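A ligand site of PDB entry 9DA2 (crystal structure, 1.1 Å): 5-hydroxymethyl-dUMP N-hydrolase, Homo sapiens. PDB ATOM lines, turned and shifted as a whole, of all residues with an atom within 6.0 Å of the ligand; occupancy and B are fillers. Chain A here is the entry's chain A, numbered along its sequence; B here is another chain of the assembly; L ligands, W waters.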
ATOM      1  N   TYR A   7     -31.914  -7.916  21.175  1.00  0.00           N
ATOM      2  CA  TYR A   7     -31.123  -8.750  20.273  1.00  0.00           C
ATOM      3  C   TYR A   7     -32.093  -9.406  19.307  1.00  0.00           C
ATOM      4  O   TYR A   7     -33.025 -10.086  19.746  1.00  0.00           O
ATOM      5  CB  TYR A   7     -30.383  -9.818  21.074  1.00  0.00           C
ATOM      6  CG  TYR A   7     -29.385 -10.655  20.299  1.00  0.00           C
ATOM      7  CD1 TYR A   7     -29.799 -11.635  19.430  1.00  0.00           C
ATOM      8  CD2 TYR A   7     -28.030 -10.475  20.475  1.00  0.00           C
ATOM      9  CE1 TYR A   7     -28.892 -12.394  18.722  1.00  0.00           C
ATOM     10  CE2 TYR A   7     -27.112 -11.228  19.794  1.00  0.00           C
ATOM     11  CZ  TYR A   7     -27.542 -12.185  18.913  1.00  0.00           C
ATOM     12  OH  TYR A   7     -26.579 -12.943  18.269  1.00  0.00           O
ATOM     13  N   PHE A   8     -31.897  -9.206  18.005  1.00  0.00           N
ATOM     14  CA  PHE A   8     -32.790  -9.752  16.984  1.00  0.00           C
ATOM     15  C   PHE A   8     -32.101 -10.880  16.228  1.00  0.00           C
ATOM     16  O   PHE A   8     -30.955 -10.737  15.783  1.00  0.00           O
ATOM     17  CB  PHE A   8     -33.266  -8.687  15.985  1.00  0.00           C
ATOM     18  CG  PHE A   8     -34.089  -9.301  14.877  1.00  0.00           C
ATOM     19  CD1 PHE A   8     -35.369  -9.738  15.143  1.00  0.00           C
ATOM     20  CD2 PHE A   8     -33.520  -9.590  13.638  1.00  0.00           C
ATOM     21  CE1 PHE A   8     -36.090 -10.406  14.167  1.00  0.00           C
ATOM     22  CE2 PHE A   8     -34.269 -10.274  12.662  1.00  0.00           C
ATOM     23  CZ  PHE A   8     -35.520 -10.671  12.930  1.00  0.00           C
ATOM     24  N   CYS A   9     -32.818 -11.993  16.053  1.00  0.00           N
ATOM     25  CA  CYS A   9     -32.358 -13.167  15.324  1.00  0.00           C
ATOM     26  C   CYS A   9     -33.263 -13.423  14.127  1.00  0.00           C
ATOM     27  O   CYS A   9     -34.480 -13.481  14.254  1.00  0.00           O
ATOM     28  CB  CYS A   9     -32.397 -14.448  16.197  1.00  0.00           C
ATOM     29  SG  CYS A   9     -31.826 -14.320  17.879  1.00  0.00           S
ATOM     30  N   GLY A  10     -32.640 -13.650  12.953  1.00  0.00           N
ATOM     31  CA  GLY A  10     -33.350 -14.083  11.764  1.00  0.00           C
ATOM     32  C   GLY A  10     -32.388 -14.672  10.765  1.00  0.00           C
ATOM     33  O   GLY A  10     -31.225 -14.261  10.700  1.00  0.00           O
ATOM     34  N   SER A  11     -32.861 -15.641   9.987  1.00  0.00           N
ATOM     35  CA  SER A  11     -32.014 -16.388   9.048  1.00  0.00           C
ATOM     36  C   SER A  11     -31.266 -15.479   8.092  1.00  0.00           C
ATOM     37  O   SER A  11     -31.826 -14.515   7.543  1.00  0.00           O
ATOM     38  CB  SER A  11     -32.930 -17.294   8.227  1.00  0.00           C
ATOM     39  OG  SER A  11     -32.215 -18.052   7.254  1.00  0.00           O
ATOM     40  N   ILE A  12     -29.986 -15.807   7.852  1.00  0.00           N
ATOM     41  CA  ILE A  12     -29.176 -15.176   6.818  1.00  0.00           C
ATOM     42  C   ILE A  12     -28.677 -16.263   5.878  1.00  0.00           C
ATOM     43  O   ILE A  12     -29.202 -16.417   4.774  1.00  0.00           O
ATOM     44  CB  ILE A  12     -28.037 -14.324   7.396  1.00  0.00           C
ATOM     45  CG1 ILE A  12     -28.625 -13.194   8.246  1.00  0.00           C
ATOM     46  CG2 ILE A  12     -27.187 -13.779   6.252  1.00  0.00           C
ATOM     47  CD1 ILE A  12     -27.578 -12.265   8.866  1.00  0.00           C
ATOM     48  N   ARG A  13     -27.710 -17.076   6.319  1.00  0.00           N
ATOM     49  CA  ARG A  13     -27.238 -18.197   5.494  1.00  0.00           C
ATOM     50  C   ARG A  13     -28.276 -19.299   5.377  1.00  0.00           C
ATOM     51  O   ARG A  13     -28.206 -20.104   4.447  1.00  0.00           O
ATOM     52  CB  ARG A  13     -25.874 -18.705   5.969  1.00  0.00           C
ATOM     53  CG  ARG A  13     -24.817 -17.628   5.742  1.00  0.00           C
ATOM     54  CD  ARG A  13     -23.439 -18.071   6.071  1.00  0.00           C
ATOM     55  NE  ARG A  13     -22.489 -16.962   6.043  1.00  0.00           N
ATOM     56  CZ  ARG A  13     -21.295 -16.999   6.608  1.00  0.00           C
ATOM     57  NH1 ARG A  13     -20.823 -18.095   7.141  1.00  0.00           N
ATOM     58  NH2 ARG A  13     -20.554 -15.884   6.650  1.00  0.00           N
ATOM     59  N   GLY A  14     -29.265 -19.353   6.270  1.00  0.00           N
ATOM     60  CA  GLY A  14     -30.375 -20.244   6.042  1.00  0.00           C
ATOM     61  C   GLY A  14     -31.245 -19.820   4.881  1.00  0.00           C
ATOM     62  O   GLY A  14     -32.058 -20.620   4.383  1.00  0.00           O
ATOM     63  N   GLY A  15     -31.081 -18.607   4.410  1.00  0.00           N
ATOM     64  CA  GLY A  15     -31.906 -18.019   3.380  1.00  0.00           C
ATOM     65  C   GLY A  15     -32.454 -16.681   3.844  1.00  0.00           C
ATOM     66  O   GLY A  15     -32.787 -16.503   5.027  1.00  0.00           O
ATOM     67  N   ASP A  56     -15.855 -15.674  10.476  1.00  0.00           N
ATOM     68  CA  ASP A  56     -16.999 -16.187  11.223  1.00  0.00           C
ATOM     69  C   ASP A  56     -16.734 -16.213  12.724  1.00  0.00           C
ATOM     70  O   ASP A  56     -17.669 -16.062  13.518  1.00  0.00           O
ATOM     71  CB  ASP A  56     -17.412 -17.563  10.687  1.00  0.00           C
ATOM     72  CG  ASP A  56     -18.032 -17.495   9.268  1.00  0.00           C
ATOM     73  OD1 ASP A  56     -18.279 -16.397   8.741  1.00  0.00           O
ATOM     74  OD2 ASP A  56     -18.312 -18.574   8.718  1.00  0.00           O
ATOM     75  N   ILE A  59     -17.766 -12.896  14.197  1.00  0.00           N
ATOM     76  CA  ILE A  59     -19.220 -12.822  14.230  1.00  0.00           C
ATOM     77  C   ILE A  59     -19.761 -13.548  15.451  1.00  0.00           C
ATOM     78  O   ILE A  59     -20.573 -13.008  16.211  1.00  0.00           O
ATOM     79  CB  ILE A  59     -19.809 -13.392  12.923  1.00  0.00           C
ATOM     80  CG1 ILE A  59     -19.492 -12.487  11.738  1.00  0.00           C
ATOM     81  CG2 ILE A  59     -21.301 -13.568  13.065  1.00  0.00           C
ATOM     82  CD1 ILE A  59     -19.824 -13.088  10.388  1.00  0.00           C
ATOM     83  N   ASP A  63     -21.470 -11.604  18.645  1.00  0.00           N
ATOM     84  CA  ASP A  63     -22.870 -11.906  18.901  1.00  0.00           C
ATOM     85  C   ASP A  63     -23.055 -12.458  20.297  1.00  0.00           C
ATOM     86  O   ASP A  63     -24.028 -12.106  20.991  1.00  0.00           O
ATOM     87  CB  ASP A  63     -23.391 -12.916  17.888  1.00  0.00           C
ATOM     88  CG  ASP A  63     -23.646 -12.324  16.528  1.00  0.00           C
ATOM     89  OD1 ASP A  63     -23.489 -11.132  16.298  1.00  0.00           O
ATOM     90  OD2 ASP A  63     -24.023 -13.164  15.650  1.00  0.00           O
ATOM     91  N   PRO A  80     -36.074 -21.853   8.489  1.00  0.00           N
ATOM     92  CA  PRO A  80     -35.110 -22.660   9.255  1.00  0.00           C
ATOM     93  C   PRO A  80     -33.693 -22.143   9.119  1.00  0.00           C
ATOM     94  O   PRO A  80     -33.238 -21.795   8.035  1.00  0.00           O
ATOM     95  CB  PRO A  80     -35.277 -24.075   8.682  1.00  0.00           C
ATOM     96  CG  PRO A  80     -36.708 -24.072   8.184  1.00  0.00           C
ATOM     97  CD  PRO A  80     -36.882 -22.691   7.604  1.00  0.00           C
ATOM     98  N   SER A  81     -32.957 -22.141  10.223  1.00  0.00           N
ATOM     99  CA  SER A  81     -31.617 -21.568  10.270  1.00  0.00           C
ATOM    100  C   SER A  81     -30.832 -22.142  11.429  1.00  0.00           C
ATOM    101  O   SER A  81     -31.297 -22.114  12.582  1.00  0.00           O
ATOM    102  CB  SER A  81     -31.733 -20.044  10.453  1.00  0.00           C
ATOM    103  OG  SER A  81     -30.507 -19.480  10.929  1.00  0.00           O
ATOM    104  N   LEU A  82     -29.637 -22.656  11.133  1.00  0.00           N
ATOM    105  CA  LEU A  82     -28.778 -23.127  12.221  1.00  0.00           C
ATOM    106  C   LEU A  82     -28.407 -21.992  13.158  1.00  0.00           C
ATOM    107  O   LEU A  82     -28.356 -22.175  14.385  1.00  0.00           O
ATOM    108  CB  LEU A  82     -27.495 -23.714  11.665  1.00  0.00           C
ATOM    109  CG  LEU A  82     -27.635 -24.975  10.803  1.00  0.00           C
ATOM    110  CD1 LEU A  82     -26.337 -25.186  10.054  1.00  0.00           C
ATOM    111  CD2 LEU A  82     -27.996 -26.208  11.628  1.00  0.00           C
ATOM    112  N   GLY A  83     -28.069 -20.826  12.603  1.00  0.00           N
ATOM    113  CA  GLY A  83     -27.571 -19.743  13.436  1.00  0.00           C
ATOM    114  C   GLY A  83     -28.629 -19.214  14.389  1.00  0.00           C
ATOM    115  O   GLY A  83     -28.337 -18.943  15.564  1.00  0.00           O
ATOM    116  N   VAL A  84     -29.874 -19.073  13.910  1.00  0.00           N
ATOM    117  CA  VAL A  84     -30.962 -18.647  14.780  1.00  0.00           C
ATOM    118  C   VAL A  84     -31.192 -19.680  15.870  1.00  0.00           C
ATOM    119  O   VAL A  84     -31.344 -19.334  17.054  1.00  0.00           O
ATOM    120  CB  VAL A  84     -32.246 -18.409  13.947  1.00  0.00           C
ATOM    121  CG1 VAL A  84     -33.444 -18.125  14.874  1.00  0.00           C
ATOM    122  CG2 VAL A  84     -32.058 -17.271  12.979  1.00  0.00           C
ATOM    123  N   GLU A  87     -28.318 -19.335  18.418  1.00  0.00           N
ATOM    124  CA  GLU A  87     -28.519 -18.159  19.249  1.00  0.00           C
ATOM    125  C   GLU A  87     -29.566 -18.424  20.329  1.00  0.00           C
ATOM    126  O   GLU A  87     -29.377 -18.054  21.487  1.00  0.00           O
ATOM    127  CB  GLU A  87     -28.956 -16.970  18.381  1.00  0.00           C
ATOM    128  CG  GLU A  87     -27.834 -16.394  17.528  1.00  0.00           C
ATOM    129  CD  GLU A  87     -28.303 -15.366  16.487  1.00  0.00           C
ATOM    130  OE1 GLU A  87     -29.343 -15.600  15.837  1.00  0.00           O
ATOM    131  OE2 GLU A  87     -27.617 -14.337  16.302  1.00  0.00           O
ATOM    132  N   LEU B 110     -21.917 -22.527   5.063  1.00  0.00           N
ATOM    133  CA  LEU B 110     -22.365 -22.897   6.412  1.00  0.00           C
ATOM    134  C   LEU B 110     -22.484 -21.657   7.289  1.00  0.00           C
ATOM    135  O   LEU B 110     -21.607 -20.783   7.294  1.00  0.00           O
ATOM    136  CB  LEU B 110     -21.357 -23.866   7.048  1.00  0.00           C
ATOM    137  CG  LEU B 110     -21.589 -24.275   8.505  1.00  0.00           C
ATOM    138  CD1 LEU B 110     -22.910 -24.984   8.662  1.00  0.00           C
ATOM    139  CD2 LEU B 110     -20.447 -25.134   9.023  1.00  0.00           C
ATOM    140  N   SER B 111     -23.566 -21.613   8.075  1.00  0.00           N
ATOM    141  CA  SER B 111     -23.781 -20.606   9.110  1.00  0.00           C
ATOM    142  C   SER B 111     -22.505 -20.155   9.805  1.00  0.00           C
ATOM    143  O   SER B 111     -21.745 -20.978  10.330  1.00  0.00           O
ATOM    144  CB  SER B 111     -24.675 -21.225  10.174  1.00  0.00           C
ATOM    145  OG  SER B 111     -24.928 -20.290  11.210  1.00  0.00           O
ATOM    146  N   ALA B 112     -22.332 -18.828   9.916  1.00  0.00           N
ATOM    147  CA  ALA B 112     -21.208 -18.281  10.668  1.00  0.00           C
ATOM    148  C   ALA B 112     -21.292 -18.649  12.144  1.00  0.00           C
ATOM    149  O   ALA B 112     -20.259 -18.716  12.810  1.00  0.00           O
ATOM    150  CB  ALA B 112     -21.150 -16.763  10.526  1.00  0.00           C
ATOM    151  N   MET B 113     -22.491 -18.882  12.682  1.00  0.00           N
ATOM    152  CA  MET B 113     -22.608 -19.203  14.099  1.00  0.00           C
ATOM    153  C   MET B 113     -21.997 -20.565  14.388  1.00  0.00           C
ATOM    154  O   MET B 113     -21.450 -20.779  15.476  1.00  0.00           O
ATOM    155  CB  MET B 113     -24.058 -19.159  14.540  1.00  0.00           C
ATOM    156  CG  MET B 113     -24.685 -17.784  14.280  1.00  0.00           C
ATOM    157  SD  MET B 113     -23.750 -16.374  14.910  1.00  0.00           S
ATOM    158  CE  MET B 113     -23.841 -16.689  16.633  1.00  0.00           C
HETATM  159  C1  LIG L   1     -28.760 -14.316  12.747  1.00  0.00           C
HETATM  160  C2  LIG L   1     -28.276 -15.725  12.614  1.00  0.00           C
HETATM  161  C3  LIG L   1     -28.397 -16.234  11.203  1.00  0.00           C
HETATM  162  C4  LIG L   1     -26.345 -14.430  13.236  1.00  0.00           C
HETATM  163  C5  LIG L   1     -24.661 -12.837  12.177  1.00  0.00           C
HETATM  164  C6  LIG L   1     -23.773 -13.340  10.125  1.00  0.00           C
HETATM  165  C7  LIG L   1     -24.411 -14.692  10.103  1.00  0.00           C
HETATM  166  C8  LIG L   1     -24.147 -15.561   8.863  1.00  0.00           C
HETATM  167  C9  LIG L   1     -25.137 -15.010  10.952  1.00  0.00           C
HETATM  168  C10 LIG L   1     -27.565 -13.553  13.110  1.00  0.00           C
HETATM  169  F1  LIG L   1     -27.365 -12.640  12.053  1.00  0.00           F
HETATM  170  N1  LIG L   1     -25.436 -14.228  12.198  1.00  0.00           N
HETATM  171  N2  LIG L   1     -23.866 -12.500  10.980  1.00  0.00           N
HETATM  172  O1  LIG L   1     -29.829 -14.167  13.695  1.00  0.00           O
HETATM  173  O2  LIG L   1     -27.867 -17.555  11.126  1.00  0.00           O
HETATM  174  O3  LIG L   1     -26.768 -17.392   8.859  1.00  0.00           O
HETATM  175  O4  LIG L   1     -27.221 -19.610  10.002  1.00  0.00           O
HETATM  176  O5  LIG L   1     -29.080 -18.244   9.020  1.00  0.00           O
HETATM  177  O6  LIG L   1     -26.873 -15.761  13.068  1.00  0.00           O
HETATM  178  O7  LIG L   1     -24.255 -16.917   9.181  1.00  0.00           O
HETATM  179  O8  LIG L   1     -23.073 -12.978   9.205  1.00  0.00           O
HETATM  180  O9  LIG L   1     -24.864 -12.147  13.131  1.00  0.00           O
HETATM  181  P1  LIG L   1     -27.722 -18.246   9.659  1.00  0.00           P
HETATM  182  O   HOH W   1     -28.312 -21.857   8.705  1.00  0.00           O
HETATM  183  O   HOH W   2     -29.814 -10.432  13.037  1.00  0.00           O
HETATM  184  O   HOH W   3     -22.830 -10.069  11.383  1.00  0.00           O
HETATM  185  O   HOH W   4     -28.290 -11.659  15.675  1.00  0.00           O
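O1 of the ligand is in hydrogen-bond range of OE1 of Glu 87 (2.6 Å). The side-chain hydroxyl of Ser 111 of chain B is in hydrogen-bond range of an oxygen (O4) of the ligand (2.7 Å). OG of Ser 81 lies within hydrogen-bond range of O5 of the ligand (2.7 Å). The backbone NH (N) of Arg 13 is in hydrogen-bond range of an oxygen (O3) of the ligand (2.7 Å). The backbone NH (N) of Ala 112 of chain B is in hydrogen-bond range of an oxygen (O7) of the ligand. The backbone NH of Ile 12 sits at hydrogen-bond distance from an oxygen (O5) of the ligand. O1 of the ligand lies within hydrogen-bond range of N of Gly 10 (3.0 Å). O1 of the ligand lies close to O of Gly 10, 3.3 Å away. N of Gly 14 is in hydrogen-bond range of O5 of the ligand (3.0 Å). The backbone NH (N) of Gly 83 lies within hydrogen-bond range of an oxygen (O4) of the ligand.
OE1 of Glu 87 sits close to SG of Cys 9 (3.5 Å). The side-chain hydroxyl (OG) of Ser 111 of chain B lies within hydrogen-bond range of the backbone NH (N) of Gly 83, 3.5 Å away. The backbone NH (N) of Met 113 of chain B sits close to the side-chain hydroxyl (OG) of Ser 111 of chain B, at 3.2 Å. The backbone NH (N) of Gly 83 sits at hydrogen-bond distance from the side-chain hydroxyl (OG) of Ser 81 (3.2 Å). OG of Ser 81 is in hydrogen-bond range of N of Val 84, 3.1 Å away. The backbone carbonyl oxygen of Leu 110 of chain B sits at hydrogen-bond distance from the guanidinium group of Arg 13 (2.8 Å). N of Gly 14 lies close to OG of Ser 11 (3.4 Å). The backbone carbonyl oxygen of Gly 15 is in hydrogen-bond range of the side-chain hydroxyl of Ser 11, at 2.8 Å.
The side-chain carboxylate (OD2) of Asp 63 lies close to an oxygen (O9) of the ligand (2.8 Å). SD of Met 113 of chain B lies close to O6 of the ligand. Residues that only touch the ligand: Cys 9 (3.2 Å), Ser 11 (3.5 Å), Ile 59 (3.5 Å) and Val 84 (3.8 Å). Hydrophobic or aromatic side chains that line the ligand: Ile 12, Ile 59, Val 84, Ala 112 of chain B and Met 113 of chain B. The nearest printed residue that does not touch the ligand is Leu 82 (4.05 Å).
Water W1 lies within hydrogen-bond range of O4 of the ligand and N of Leu 82. Water W4 lies within hydrogen-bond range of the backbone carbonyl oxygen of Phe 8 (2.8 Å), the side-chain carboxylate of Glu 87 (2.8 Å) and the side-chain hydroxyl of Tyr 7 (3.4 Å).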
